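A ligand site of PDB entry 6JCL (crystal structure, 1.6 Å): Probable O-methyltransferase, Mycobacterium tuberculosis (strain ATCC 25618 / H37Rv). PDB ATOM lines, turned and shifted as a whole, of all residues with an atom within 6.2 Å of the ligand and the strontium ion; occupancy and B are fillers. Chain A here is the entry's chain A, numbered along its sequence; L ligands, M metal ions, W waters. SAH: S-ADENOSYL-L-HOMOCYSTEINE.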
ATOM      1  N   ILE A  42      17.775 -25.711 -27.190  1.00  0.00           N
ATOM      2  CA  ILE A  42      17.443 -26.056 -25.807  1.00  0.00           C
ATOM      3  C   ILE A  42      16.640 -24.956 -25.122  1.00  0.00           C
ATOM      4  O   ILE A  42      16.599 -24.883 -23.890  1.00  0.00           O
ATOM      5  CB  ILE A  42      18.727 -26.376 -25.010  1.00  0.00           C
ATOM      6  CG1 ILE A  42      19.622 -25.134 -24.907  1.00  0.00           C
ATOM      7  CG2 ILE A  42      19.477 -27.617 -25.626  1.00  0.00           C
ATOM      8  CD1 ILE A  42      20.858 -25.332 -23.992  1.00  0.00           C
ATOM      9  N   ALA A  43      16.028 -24.068 -25.903  1.00  0.00           N
ATOM     10  CA  ALA A  43      15.188 -23.017 -25.360  1.00  0.00           C
ATOM     11  C   ALA A  43      13.950 -23.585 -24.682  1.00  0.00           C
ATOM     12  O   ALA A  43      13.548 -24.725 -24.913  1.00  0.00           O
ATOM     13  CB  ALA A  43      14.754 -22.079 -26.499  1.00  0.00           C
ATOM     14  N   VAL A  44      13.320 -22.753 -23.849  1.00  0.00           N
ATOM     15  CA  VAL A  44      12.053 -23.172 -23.265  1.00  0.00           C
ATOM     16  C   VAL A  44      11.062 -23.478 -24.382  1.00  0.00           C
ATOM     17  O   VAL A  44      11.107 -22.875 -25.464  1.00  0.00           O
ATOM     18  CB  VAL A  44      11.472 -22.098 -22.314  1.00  0.00           C
ATOM     19  CG1 VAL A  44      12.332 -21.959 -21.082  1.00  0.00           C
ATOM     20  CG2 VAL A  44      11.289 -20.761 -23.023  1.00  0.00           C
ATOM     21  N   GLU A  66      17.137 -12.500 -15.346  1.00  0.00           N
ATOM     22  CA  GLU A  66      17.291 -13.822 -15.957  1.00  0.00           C
ATOM     23  C   GLU A  66      18.769 -14.180 -16.027  1.00  0.00           C
ATOM     24  O   GLU A  66      19.604 -13.333 -16.384  1.00  0.00           O
ATOM     25  CB  GLU A  66      16.662 -13.887 -17.333  1.00  0.00           C
ATOM     26  CG  GLU A  66      16.995 -15.176 -18.083  1.00  0.00           C
ATOM     27  CD  GLU A  66      16.342 -15.174 -19.447  1.00  0.00           C
ATOM     28  OE1 GLU A  66      16.796 -14.393 -20.311  1.00  0.00           O
ATOM     29  OE2 GLU A  66      15.349 -15.919 -19.648  1.00  0.00           O
ATOM     30  N   ILE A  67      19.093 -15.411 -15.667  1.00  0.00           N
ATOM     31  CA  ILE A  67      20.469 -15.892 -15.731  1.00  0.00           C
ATOM     32  C   ILE A  67      20.489 -17.026 -16.750  1.00  0.00           C
ATOM     33  O   ILE A  67      19.920 -18.104 -16.516  1.00  0.00           O
ATOM     34  CB  ILE A  67      20.971 -16.341 -14.349  1.00  0.00           C
ATOM     35  CG1 ILE A  67      20.618 -15.269 -13.312  1.00  0.00           C
ATOM     36  CG2 ILE A  67      22.478 -16.540 -14.374  1.00  0.00           C
ATOM     37  CD1 ILE A  67      21.109 -15.584 -11.889  1.00  0.00           C
ATOM     38  N   GLY A  68      21.116 -16.780 -17.908  1.00  0.00           N
ATOM     39  CA  GLY A  68      21.183 -17.740 -19.000  1.00  0.00           C
ATOM     40  C   GLY A  68      20.273 -17.344 -20.155  1.00  0.00           C
ATOM     41  O   GLY A  68      19.114 -17.748 -20.206  1.00  0.00           O
ATOM     42  N   THR A  69      20.793 -16.557 -21.100  1.00  0.00           N
ATOM     43  CA  THR A  69      19.979 -15.959 -22.157  1.00  0.00           C
ATOM     44  C   THR A  69      19.806 -16.853 -23.369  1.00  0.00           C
ATOM     45  O   THR A  69      18.716 -16.909 -23.954  1.00  0.00           O
ATOM     46  CB  THR A  69      20.612 -14.635 -22.598  1.00  0.00           C
ATOM     47  OG1 THR A  69      20.916 -13.827 -21.454  1.00  0.00           O
ATOM     48  CG2 THR A  69      19.659 -13.827 -23.518  1.00  0.00           C
ATOM     49  N   LEU A  70      20.880 -17.553 -23.763  1.00  0.00           N
ATOM     50  CA  LEU A  70      20.965 -18.245 -25.048  1.00  0.00           C
ATOM     51  C   LEU A  70      20.583 -17.267 -26.164  1.00  0.00           C
ATOM     52  O   LEU A  70      21.222 -16.228 -26.299  1.00  0.00           O
ATOM     53  CB  LEU A  70      20.085 -19.499 -25.058  1.00  0.00           C
ATOM     54  CG  LEU A  70      20.278 -20.508 -26.204  1.00  0.00           C
ATOM     55  CD1 LEU A  70      21.735 -20.985 -26.337  1.00  0.00           C
ATOM     56  CD2 LEU A  70      19.319 -21.707 -26.072  1.00  0.00           C
ATOM     57  N   GLY A  71      19.541 -17.567 -26.940  1.00  0.00           N
ATOM     58  CA  GLY A  71      19.085 -16.699 -28.019  1.00  0.00           C
ATOM     59  C   GLY A  71      17.955 -15.781 -27.624  1.00  0.00           C
ATOM     60  O   GLY A  71      17.362 -15.137 -28.494  1.00  0.00           O
ATOM     61  N   GLY A  72      17.616 -15.703 -26.339  1.00  0.00           N
ATOM     62  CA  GLY A  72      16.576 -14.786 -25.880  1.00  0.00           C
ATOM     63  C   GLY A  72      15.152 -15.286 -25.942  1.00  0.00           C
ATOM     64  O   GLY A  72      14.223 -14.472 -25.804  1.00  0.00           O
ATOM     65  N   PHE A  73      14.920 -16.586 -26.144  1.00  0.00           N
ATOM     66  CA  PHE A  73      13.543 -17.054 -26.275  1.00  0.00           C
ATOM     67  C   PHE A  73      12.792 -16.902 -24.960  1.00  0.00           C
ATOM     68  O   PHE A  73      11.710 -16.289 -24.914  1.00  0.00           O
ATOM     69  CB  PHE A  73      13.554 -18.514 -26.768  1.00  0.00           C
ATOM     70  CG  PHE A  73      12.211 -19.066 -27.152  1.00  0.00           C
ATOM     71  CD1 PHE A  73      11.393 -19.689 -26.204  1.00  0.00           C
ATOM     72  CD2 PHE A  73      11.758 -18.992 -28.462  1.00  0.00           C
ATOM     73  CE1 PHE A  73      10.118 -20.216 -26.573  1.00  0.00           C
ATOM     74  CE2 PHE A  73      10.519 -19.516 -28.826  1.00  0.00           C
ATOM     75  CZ  PHE A  73       9.700 -20.130 -27.875  1.00  0.00           C
ATOM     76  N   SER A  74      13.365 -17.409 -23.857  1.00  0.00           N
ATOM     77  CA  SER A  74      12.738 -17.183 -22.553  1.00  0.00           C
ATOM     78  C   SER A  74      12.676 -15.693 -22.217  1.00  0.00           C
ATOM     79  O   SER A  74      11.699 -15.212 -21.634  1.00  0.00           O
ATOM     80  CB  SER A  74      13.501 -17.945 -21.450  1.00  0.00           C
ATOM     81  OG  SER A  74      14.873 -17.586 -21.433  1.00  0.00           O
ATOM     82  N   THR A  75      13.702 -14.942 -22.623  1.00  0.00           N
ATOM     83  CA  THR A  75      13.780 -13.503 -22.360  1.00  0.00           C
ATOM     84  C   THR A  75      12.636 -12.733 -23.014  1.00  0.00           C
ATOM     85  O   THR A  75      12.058 -11.821 -22.408  1.00  0.00           O
ATOM     86  CB  THR A  75      15.107 -12.976 -22.867  1.00  0.00           C
ATOM     87  OG1 THR A  75      16.129 -13.958 -22.637  1.00  0.00           O
ATOM     88  CG2 THR A  75      15.460 -11.657 -22.181  1.00  0.00           C
ATOM     89  N   LEU A  91      21.568 -12.272 -18.181  1.00  0.00           N
ATOM     90  CA  LEU A  91      23.004 -12.509 -18.074  1.00  0.00           C
ATOM     91  C   LEU A  91      23.423 -13.637 -18.995  1.00  0.00           C
ATOM     92  O   LEU A  91      22.835 -14.726 -18.966  1.00  0.00           O
ATOM     93  CB  LEU A  91      23.380 -12.859 -16.627  1.00  0.00           C
ATOM     94  CG  LEU A  91      22.895 -11.855 -15.568  1.00  0.00           C
ATOM     95  CD1 LEU A  91      23.455 -12.218 -14.193  1.00  0.00           C
ATOM     96  CD2 LEU A  91      23.245 -10.388 -15.917  1.00  0.00           C
ATOM     97  N   GLU A  92      24.468 -13.395 -19.789  1.00  0.00           N
ATOM     98  CA  GLU A  92      24.912 -14.387 -20.778  1.00  0.00           C
ATOM     99  C   GLU A  92      26.427 -14.307 -20.885  1.00  0.00           C
ATOM    100  O   GLU A  92      26.962 -13.219 -21.074  1.00  0.00           O
ATOM    101  CB  GLU A  92      24.284 -14.089 -22.146  1.00  0.00           C
ATOM    102  CG  GLU A  92      24.770 -14.994 -23.267  1.00  0.00           C
ATOM    103  CD  GLU A  92      24.643 -16.471 -22.926  1.00  0.00           C
ATOM    104  OE1 GLU A  92      23.533 -16.904 -22.510  1.00  0.00           O
ATOM    105  OE2 GLU A  92      25.658 -17.182 -23.052  1.00  0.00           O
ATOM    106  N   TYR A  93      27.129 -15.431 -20.736  1.00  0.00           N
ATOM    107  CA  TYR A  93      28.574 -15.302 -20.824  1.00  0.00           C
ATOM    108  C   TYR A  93      29.150 -15.566 -22.219  1.00  0.00           C
ATOM    109  O   TYR A  93      30.344 -15.301 -22.418  1.00  0.00           O
ATOM    110  CB  TYR A  93      29.259 -16.119 -19.717  1.00  0.00           C
ATOM    111  CG  TYR A  93      29.544 -17.569 -19.936  1.00  0.00           C
ATOM    112  CD1 TYR A  93      28.581 -18.435 -20.410  1.00  0.00           C
ATOM    113  CD2 TYR A  93      30.771 -18.100 -19.547  1.00  0.00           C
ATOM    114  CE1 TYR A  93      28.863 -19.799 -20.576  1.00  0.00           C
ATOM    115  CE2 TYR A  93      31.051 -19.440 -19.689  1.00  0.00           C
ATOM    116  CZ  TYR A  93      30.097 -20.290 -20.203  1.00  0.00           C
ATOM    117  OH  TYR A  93      30.391 -21.623 -20.329  1.00  0.00           O
ATOM    118  N   GLN A  94      28.386 -16.145 -23.158  1.00  0.00           N
ATOM    119  CA  GLN A  94      28.907 -16.363 -24.522  1.00  0.00           C
ATOM    120  C   GLN A  94      28.591 -15.149 -25.381  1.00  0.00           C
ATOM    121  O   GLN A  94      27.409 -14.916 -25.678  1.00  0.00           O
ATOM    122  CB  GLN A  94      28.275 -17.580 -25.176  1.00  0.00           C
ATOM    123  CG  GLN A  94      28.681 -18.906 -24.648  1.00  0.00           C
ATOM    124  CD  GLN A  94      30.064 -19.359 -25.103  1.00  0.00           C
ATOM    125  OE1 GLN A  94      30.727 -18.718 -25.951  1.00  0.00           O
ATOM    126  NE2 GLN A  94      30.496 -20.476 -24.549  1.00  0.00           N
ATOM    127  N   HIS A  97      26.115 -15.878 -28.232  1.00  0.00           N
ATOM    128  CA  HIS A  97      24.721 -16.008 -27.802  1.00  0.00           C
ATOM    129  C   HIS A  97      24.112 -14.626 -27.545  1.00  0.00           C
ATOM    130  O   HIS A  97      22.998 -14.332 -27.980  1.00  0.00           O
ATOM    131  CB  HIS A  97      24.627 -16.874 -26.551  1.00  0.00           C
ATOM    132  CG  HIS A  97      25.063 -18.287 -26.791  1.00  0.00           C
ATOM    133  ND1 HIS A  97      24.892 -19.291 -25.860  1.00  0.00           N
ATOM    134  CD2 HIS A  97      25.687 -18.851 -27.852  1.00  0.00           C
ATOM    135  CE1 HIS A  97      25.374 -20.418 -26.357  1.00  0.00           C
ATOM    136  NE2 HIS A  97      25.885 -20.175 -27.548  1.00  0.00           N
ATOM    137  N   GLY A 119      29.038 -11.651 -19.749  1.00  0.00           N
ATOM    138  CA  GLY A 119      30.086 -12.072 -18.854  1.00  0.00           C
ATOM    139  C   GLY A 119      29.594 -13.204 -17.983  1.00  0.00           C
ATOM    140  O   GLY A 119      28.398 -13.506 -17.918  1.00  0.00           O
ATOM    141  N   PRO A 120      30.510 -13.871 -17.280  1.00  0.00           N
ATOM    142  CA  PRO A 120      30.094 -14.898 -16.320  1.00  0.00           C
ATOM    143  C   PRO A 120      29.225 -14.270 -15.229  1.00  0.00           C
ATOM    144  O   PRO A 120      29.572 -13.232 -14.658  1.00  0.00           O
ATOM    145  CB  PRO A 120      31.431 -15.419 -15.744  1.00  0.00           C
ATOM    146  CG  PRO A 120      32.517 -14.831 -16.616  1.00  0.00           C
ATOM    147  CD  PRO A 120      31.952 -13.555 -17.181  1.00  0.00           C
ATOM    148  N   ALA A 121      28.087 -14.907 -14.966  1.00  0.00           N
ATOM    149  CA  ALA A 121      27.109 -14.329 -14.038  1.00  0.00           C
ATOM    150  C   ALA A 121      27.676 -14.094 -12.647  1.00  0.00           C
ATOM    151  O   ALA A 121      27.264 -13.155 -11.967  1.00  0.00           O
ATOM    152  CB  ALA A 121      25.860 -15.211 -13.962  1.00  0.00           C
ATOM    153  N   LEU A 122      28.594 -14.954 -12.179  1.00  0.00           N
ATOM    154  CA  LEU A 122      29.185 -14.719 -10.866  1.00  0.00           C
ATOM    155  C   LEU A 122      29.960 -13.421 -10.813  1.00  0.00           C
ATOM    156  O   LEU A 122      30.149 -12.857  -9.719  1.00  0.00           O
ATOM    157  CB  LEU A 122      30.114 -15.876 -10.491  1.00  0.00           C
ATOM    158  CG  LEU A 122      29.452 -17.209 -10.095  1.00  0.00           C
ATOM    159  CD1 LEU A 122      30.510 -18.283  -9.864  1.00  0.00           C
ATOM    160  CD2 LEU A 122      28.571 -17.040  -8.872  1.00  0.00           C
ATOM    161  N   PHE A 137      14.602 -15.697 -13.012  1.00  0.00           N
ATOM    162  CA  PHE A 137      14.570 -16.980 -13.738  1.00  0.00           C
ATOM    163  C   PHE A 137      15.988 -17.477 -13.858  1.00  0.00           C
ATOM    164  O   PHE A 137      16.827 -16.806 -14.466  1.00  0.00           O
ATOM    165  CB  PHE A 137      13.932 -16.807 -15.119  1.00  0.00           C
ATOM    166  CG  PHE A 137      13.893 -18.080 -15.931  1.00  0.00           C
ATOM    167  CD1 PHE A 137      13.442 -19.275 -15.368  1.00  0.00           C
ATOM    168  CD2 PHE A 137      14.304 -18.079 -17.257  1.00  0.00           C
ATOM    169  CE1 PHE A 137      13.408 -20.471 -16.153  1.00  0.00           C
ATOM    170  CE2 PHE A 137      14.273 -19.248 -18.026  1.00  0.00           C
ATOM    171  CZ  PHE A 137      13.824 -20.453 -17.466  1.00  0.00           C
ATOM    172  N   ASP A 139      18.571 -20.142 -15.224  1.00  0.00           N
ATOM    173  CA  ASP A 139      18.638 -21.134 -16.289  1.00  0.00           C
ATOM    174  C   ASP A 139      20.004 -21.077 -16.991  1.00  0.00           C
ATOM    175  O   ASP A 139      20.089 -21.017 -18.218  1.00  0.00           O
ATOM    176  CB  ASP A 139      17.494 -20.924 -17.286  1.00  0.00           C
ATOM    177  CG  ASP A 139      17.347 -22.111 -18.252  1.00  0.00           C
ATOM    178  OD1 ASP A 139      17.757 -23.239 -17.850  1.00  0.00           O
ATOM    179  OD2 ASP A 139      16.843 -21.924 -19.394  1.00  0.00           O
ATOM    180  N   ALA A 140      21.086 -21.123 -16.222  1.00  0.00           N
ATOM    181  CA  ALA A 140      22.420 -20.997 -16.805  1.00  0.00           C
ATOM    182  C   ALA A 140      23.251 -22.260 -16.554  1.00  0.00           C
ATOM    183  O   ALA A 140      22.760 -23.363 -16.829  1.00  0.00           O
ATOM    184  CB  ALA A 140      23.107 -19.722 -16.288  1.00  0.00           C
ATOM    185  N   ASP A 141      24.482 -22.129 -16.034  1.00  0.00           N
ATOM    186  CA  ASP A 141      25.311 -23.305 -15.700  1.00  0.00           C
ATOM    187  C   ASP A 141      24.817 -23.922 -14.395  1.00  0.00           C
ATOM    188  O   ASP A 141      24.723 -23.229 -13.373  1.00  0.00           O
ATOM    189  CB  ASP A 141      26.794 -22.937 -15.609  1.00  0.00           C
ATOM    190  CG  ASP A 141      27.062 -21.726 -14.725  1.00  0.00           C
ATOM    191  OD1 ASP A 141      26.266 -20.771 -14.742  1.00  0.00           O
ATOM    192  OD2 ASP A 141      28.091 -21.741 -14.029  1.00  0.00           O
ATOM    193  N   LYS A 142      24.457 -25.213 -14.436  1.00  0.00           N
ATOM    194  CA  LYS A 142      23.683 -25.775 -13.320  1.00  0.00           C
ATOM    195  C   LYS A 142      24.489 -25.868 -12.036  1.00  0.00           C
ATOM    196  O   LYS A 142      23.894 -25.793 -10.949  1.00  0.00           O
ATOM    197  CB  LYS A 142      23.139 -27.164 -13.683  1.00  0.00           C
ATOM    198  CG  LYS A 142      22.309 -27.186 -14.959  1.00  0.00           C
ATOM    199  CD  LYS A 142      21.226 -26.097 -14.978  1.00  0.00           C
ATOM    200  CE  LYS A 142      20.187 -26.364 -16.075  1.00  0.00           C
ATOM    201  NZ  LYS A 142      19.376 -25.131 -16.324  1.00  0.00           N
ATOM    202  N   ASN A 144      26.140 -23.734 -10.708  1.00  0.00           N
ATOM    203  CA  ASN A 144      26.028 -22.491  -9.956  1.00  0.00           C
ATOM    204  C   ASN A 144      24.595 -22.126  -9.602  1.00  0.00           C
ATOM    205  O   ASN A 144      24.352 -21.016  -9.116  1.00  0.00           O
ATOM    206  CB  ASN A 144      26.682 -21.345 -10.720  1.00  0.00           C
ATOM    207  CG  ASN A 144      28.157 -21.197 -10.390  1.00  0.00           C
ATOM    208  OD1 ASN A 144      28.555 -21.248  -9.217  1.00  0.00           O
ATOM    209  ND2 ASN A 144      28.964 -20.989 -11.409  1.00  0.00           N
ATOM    210  N   TYR A 148      23.566 -18.745  -7.644  1.00  0.00           N
ATOM    211  CA  TYR A 148      22.638 -17.794  -8.274  1.00  0.00           C
ATOM    212  C   TYR A 148      21.398 -17.590  -7.419  1.00  0.00           C
ATOM    213  O   TYR A 148      20.840 -16.484  -7.381  1.00  0.00           O
ATOM    214  CB  TYR A 148      22.251 -18.276  -9.685  1.00  0.00           C
ATOM    215  CG  TYR A 148      23.419 -18.374 -10.622  1.00  0.00           C
ATOM    216  CD1 TYR A 148      24.545 -17.569 -10.446  1.00  0.00           C
ATOM    217  CD2 TYR A 148      23.405 -19.262 -11.678  1.00  0.00           C
ATOM    218  CE1 TYR A 148      25.632 -17.666 -11.298  1.00  0.00           C
ATOM    219  CE2 TYR A 148      24.480 -19.370 -12.533  1.00  0.00           C
ATOM    220  CZ  TYR A 148      25.584 -18.562 -12.345  1.00  0.00           C
ATOM    221  OH  TYR A 148      26.660 -18.679 -13.203  1.00  0.00           O
ATOM    222  N   ASP A 165      14.937 -23.667 -13.730  1.00  0.00           N
ATOM    223  CA  ASP A 165      14.612 -24.629 -14.783  1.00  0.00           C
ATOM    224  C   ASP A 165      15.422 -25.935 -14.628  1.00  0.00           C
ATOM    225  O   ASP A 165      16.529 -25.955 -14.064  1.00  0.00           O
ATOM    226  CB  ASP A 165      14.896 -24.023 -16.164  1.00  0.00           C
ATOM    227  CG  ASP A 165      14.100 -24.702 -17.279  1.00  0.00           C
ATOM    228  OD1 ASP A 165      13.066 -25.352 -16.972  1.00  0.00           O
ATOM    229  OD2 ASP A 165      14.499 -24.572 -18.466  1.00  0.00           O
ATOM    230  N   ASN A 166      14.849 -27.020 -15.151  1.00  0.00           N
ATOM    231  CA  ASN A 166      15.563 -28.285 -15.370  1.00  0.00           C
ATOM    232  C   ASN A 166      15.984 -28.974 -14.065  1.00  0.00           C
ATOM    233  O   ASN A 166      17.097 -29.496 -13.969  1.00  0.00           O
ATOM    234  CB  ASN A 166      16.812 -28.101 -16.255  1.00  0.00           C
ATOM    235  CG  ASN A 166      16.530 -27.380 -17.566  1.00  0.00           C
ATOM    236  OD1 ASN A 166      17.061 -26.292 -17.814  1.00  0.00           O
ATOM    237  ND2 ASN A 166      15.705 -27.999 -18.421  1.00  0.00           N
ATOM    238  N   LYS A 209      10.058 -31.333 -24.559  1.00  0.00           N
ATOM    239  CA  LYS A 209      11.424 -31.478 -24.087  1.00  0.00           C
ATOM    240  C   LYS A 209      11.643 -32.698 -23.188  1.00  0.00           C
ATOM    241  O   LYS A 209      12.759 -32.888 -22.687  1.00  0.00           O
ATOM    242  CB  LYS A 209      11.849 -30.190 -23.352  1.00  0.00           C
ATOM    243  CG  LYS A 209      11.770 -28.957 -24.263  1.00  0.00           C
ATOM    244  CD  LYS A 209      12.208 -27.693 -23.516  1.00  0.00           C
ATOM    245  CE  LYS A 209      13.653 -27.821 -23.092  1.00  0.00           C
ATOM    246  NZ  LYS A 209      14.177 -26.504 -22.541  1.00  0.00           N
HETATM  247  N   SAH L   1      16.953 -19.443 -20.932  1.00  0.00           N
HETATM  248  CA  SAH L   1      17.185 -19.803 -22.335  1.00  0.00           C
HETATM  249  CB  SAH L   1      18.145 -20.976 -22.422  1.00  0.00           C
HETATM  250  CG  SAH L   1      19.454 -20.780 -21.647  1.00  0.00           C
HETATM  251  SD  SAH L   1      20.631 -22.073 -22.113  1.00  0.00           S
HETATM  252  C   SAH L   1      15.879 -20.132 -23.044  1.00  0.00           C
HETATM  253  O   SAH L   1      15.582 -19.634 -24.138  1.00  0.00           O
HETATM  254  OXT SAH L   1      15.086 -20.884 -22.493  1.00  0.00           O
HETATM  255  C5' SAH L   1      21.894 -21.666 -20.880  1.00  0.00           C
HETATM  256  C4' SAH L   1      22.694 -20.406 -21.205  1.00  0.00           C
HETATM  257  O4' SAH L   1      23.491 -20.094 -20.085  1.00  0.00           O
HETATM  258  C3' SAH L   1      23.674 -20.546 -22.384  1.00  0.00           C
HETATM  259  O3' SAH L   1      23.428 -19.489 -23.315  1.00  0.00           O
HETATM  260  C2' SAH L   1      25.054 -20.402 -21.757  1.00  0.00           C
HETATM  261  O2' SAH L   1      26.027 -19.823 -22.618  1.00  0.00           O
HETATM  262  C1' SAH L   1      24.730 -19.575 -20.516  1.00  0.00           C
HETATM  263  N9  SAH L   1      25.731 -19.664 -19.429  1.00  0.00           N
HETATM  264  C8  SAH L   1      26.439 -20.779 -19.042  1.00  0.00           C
HETATM  265  N7  SAH L   1      27.236 -20.413 -18.009  1.00  0.00           N
HETATM  266  C5  SAH L   1      27.019 -19.101 -17.741  1.00  0.00           C
HETATM  267  C6  SAH L   1      27.597 -18.245 -16.802  1.00  0.00           C
HETATM  268  N6  SAH L   1      28.529 -18.669 -15.939  1.00  0.00           N
HETATM  269  N1  SAH L   1      27.165 -16.938 -16.767  1.00  0.00           N
HETATM  270  C2  SAH L   1      26.217 -16.471 -17.666  1.00  0.00           C
HETATM  271  N3  SAH L   1      25.667 -17.322 -18.607  1.00  0.00           N
HETATM  272  C4  SAH L   1      26.077 -18.616 -18.627  1.00  0.00           C
HETATM  273 SR    SR M   1      16.661 -24.530 -19.653  1.00  0.00          SR
HETATM  274  O   HOH W   1      25.691 -23.674 -20.690  1.00  0.00           O
HETATM  275  O   HOH W   2      15.540 -23.618 -21.748  1.00  0.00           O
HETATM  276  O   HOH W   3      30.533 -20.619 -14.925  1.00  0.00           O
HETATM  277  O   HOH W   4      27.744 -21.613 -23.606  1.00  0.00           O
HETATM  278  O   HOH W   5      16.906 -18.818 -26.460  1.00  0.00           O
HETATM  279  O   HOH W   6      29.379 -17.428 -13.368  1.00  0.00           O
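N of the ligand lies close to OD2 of Asp 139, 2.9 Å away.
OE2 of Glu 92 sits at hydrogen-bond distance from O2' of the ligand (2.7 Å).
The backbone NH (N) of Ser 74 lies within hydrogen-bond range of an oxygen (O) of the ligand, at 3.2 Å.
A nitrogen (N) of the ligand lies within hydrogen-bond range of the side-chain hydroxyl of Ser 74 (2.8 Å).
N of the ligand sits at hydrogen-bond distance from O of Gly 68, at 2.8 Å.
N of Ala 121 lies within hydrogen-bond range of N1 of the ligand.
The backbone NH (N) of Val 44 lies within hydrogen-bond range of an oxygen (OXT) of the ligand, at 2.9 Å.
O3' of the ligand lies within hydrogen-bond range of ND1 of His 97, at 2.9 Å.
The backbone NH (N) of Tyr 93 lies within hydrogen-bond range of a nitrogen (N3) of the ligand, 3.2 Å away.
N of Leu 70 lies within hydrogen-bond range of O3' of the ligand, 3.2 Å away.
A nitrogen (N6) of the ligand sits at hydrogen-bond distance from the side-chain carboxylate of Asp 141 (3.3 Å).
N6 of the ligand lies within hydrogen-bond range of OH of Tyr 148.
The side-chain amino group (NZ) of Lys 142 lies close to the side-chain amide oxygen (OD1) of Asn 166 (3.0 Å).
OE1 of Glu 92 is in hydrogen-bond range of N of Leu 70 (3.0 Å).
OE1 of Glu 92 lies within hydrogen-bond range of N of Thr 69.
The side-chain hydroxyl (OH) of Tyr 148 lies within hydrogen-bond range of the side-chain carboxylate (OD1) of Asp 141 (2.6 Å).
The side-chain carboxylate (OD2) of Asp 141 sits at hydrogen-bond distance from the side-chain amide nitrogen (ND2) of Asn 144 (2.9 Å).
The backbone carbonyl oxygen of Ala 43 sits at hydrogen-bond distance from the side-chain amino group of Lys 209 (3.0 Å).
The side-chain hydroxyl (OG1) of Thr 69 lies within hydrogen-bond range of the backbone carbonyl oxygen (O) of Leu 91, 3.3 Å away.
The side-chain amino group (NZ) of Lys 209 lies within hydrogen-bond range of the backbone carbonyl oxygen (O) of Ile 42, 3.2 Å away.
Merely in contact with the ligand: Ile 42, Ala 43, Thr 69, Phe 73, Leu 91, Gln 94, Gly 119, Pro 120, Phe 137 and Ala 140.
Hydrophobic or aromatic side chains that line the ligand: Ile 42, Ala 43, Val 44, Leu 70, Phe 73, Tyr 93, His 97, Ala 121, Phe 137 and Ala 140.
21 residues have an atom within 4 Å of the ligand: Ile 42, Ala 43, Val 44, Gly 68, Thr 69, Leu 70, Phe 73, Ser 74, Leu 91, Glu 92, Tyr 93, Gln 94, His 97, Gly 119, Pro 120, Ala 121, Phe 137, Asp 139, Ala 140, Asp 141 and Tyr 148.
The nearest printed residue that does not touch the ligand is Glu 66 (4.1 Å).
Within 4 Å of the strontium ion: Asp 139, Asp 165 and Asn 166.
Along chain A the residues within 4 Å of the strontium ion span positions 139 to 166.
The nearest printed residue that does not touch the strontium ion is Ile 42 (4.3 Å).
The strontium ion is bound by OD2 of Asp 165 (2.5 Å), OD1 of Asp 139 (2.5 Å), water W2 (2.5 Å), OD1 of Asn 166 (2.6 Å) and OD2 of Asp 139 (2.6 Å).
Water W2 lies within hydrogen-bond range of O of Ile 42, OXT of the ligand, N of Val 44 and NZ of Lys 209.
Water W4 bridges O2' of the ligand (2.7 Å) and NE2 of Gln 94 (3.1 Å).
Water W3 bridges OD2 of Asp 141 (2.8 Å) and N6 of the ligand (3.0 Å).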
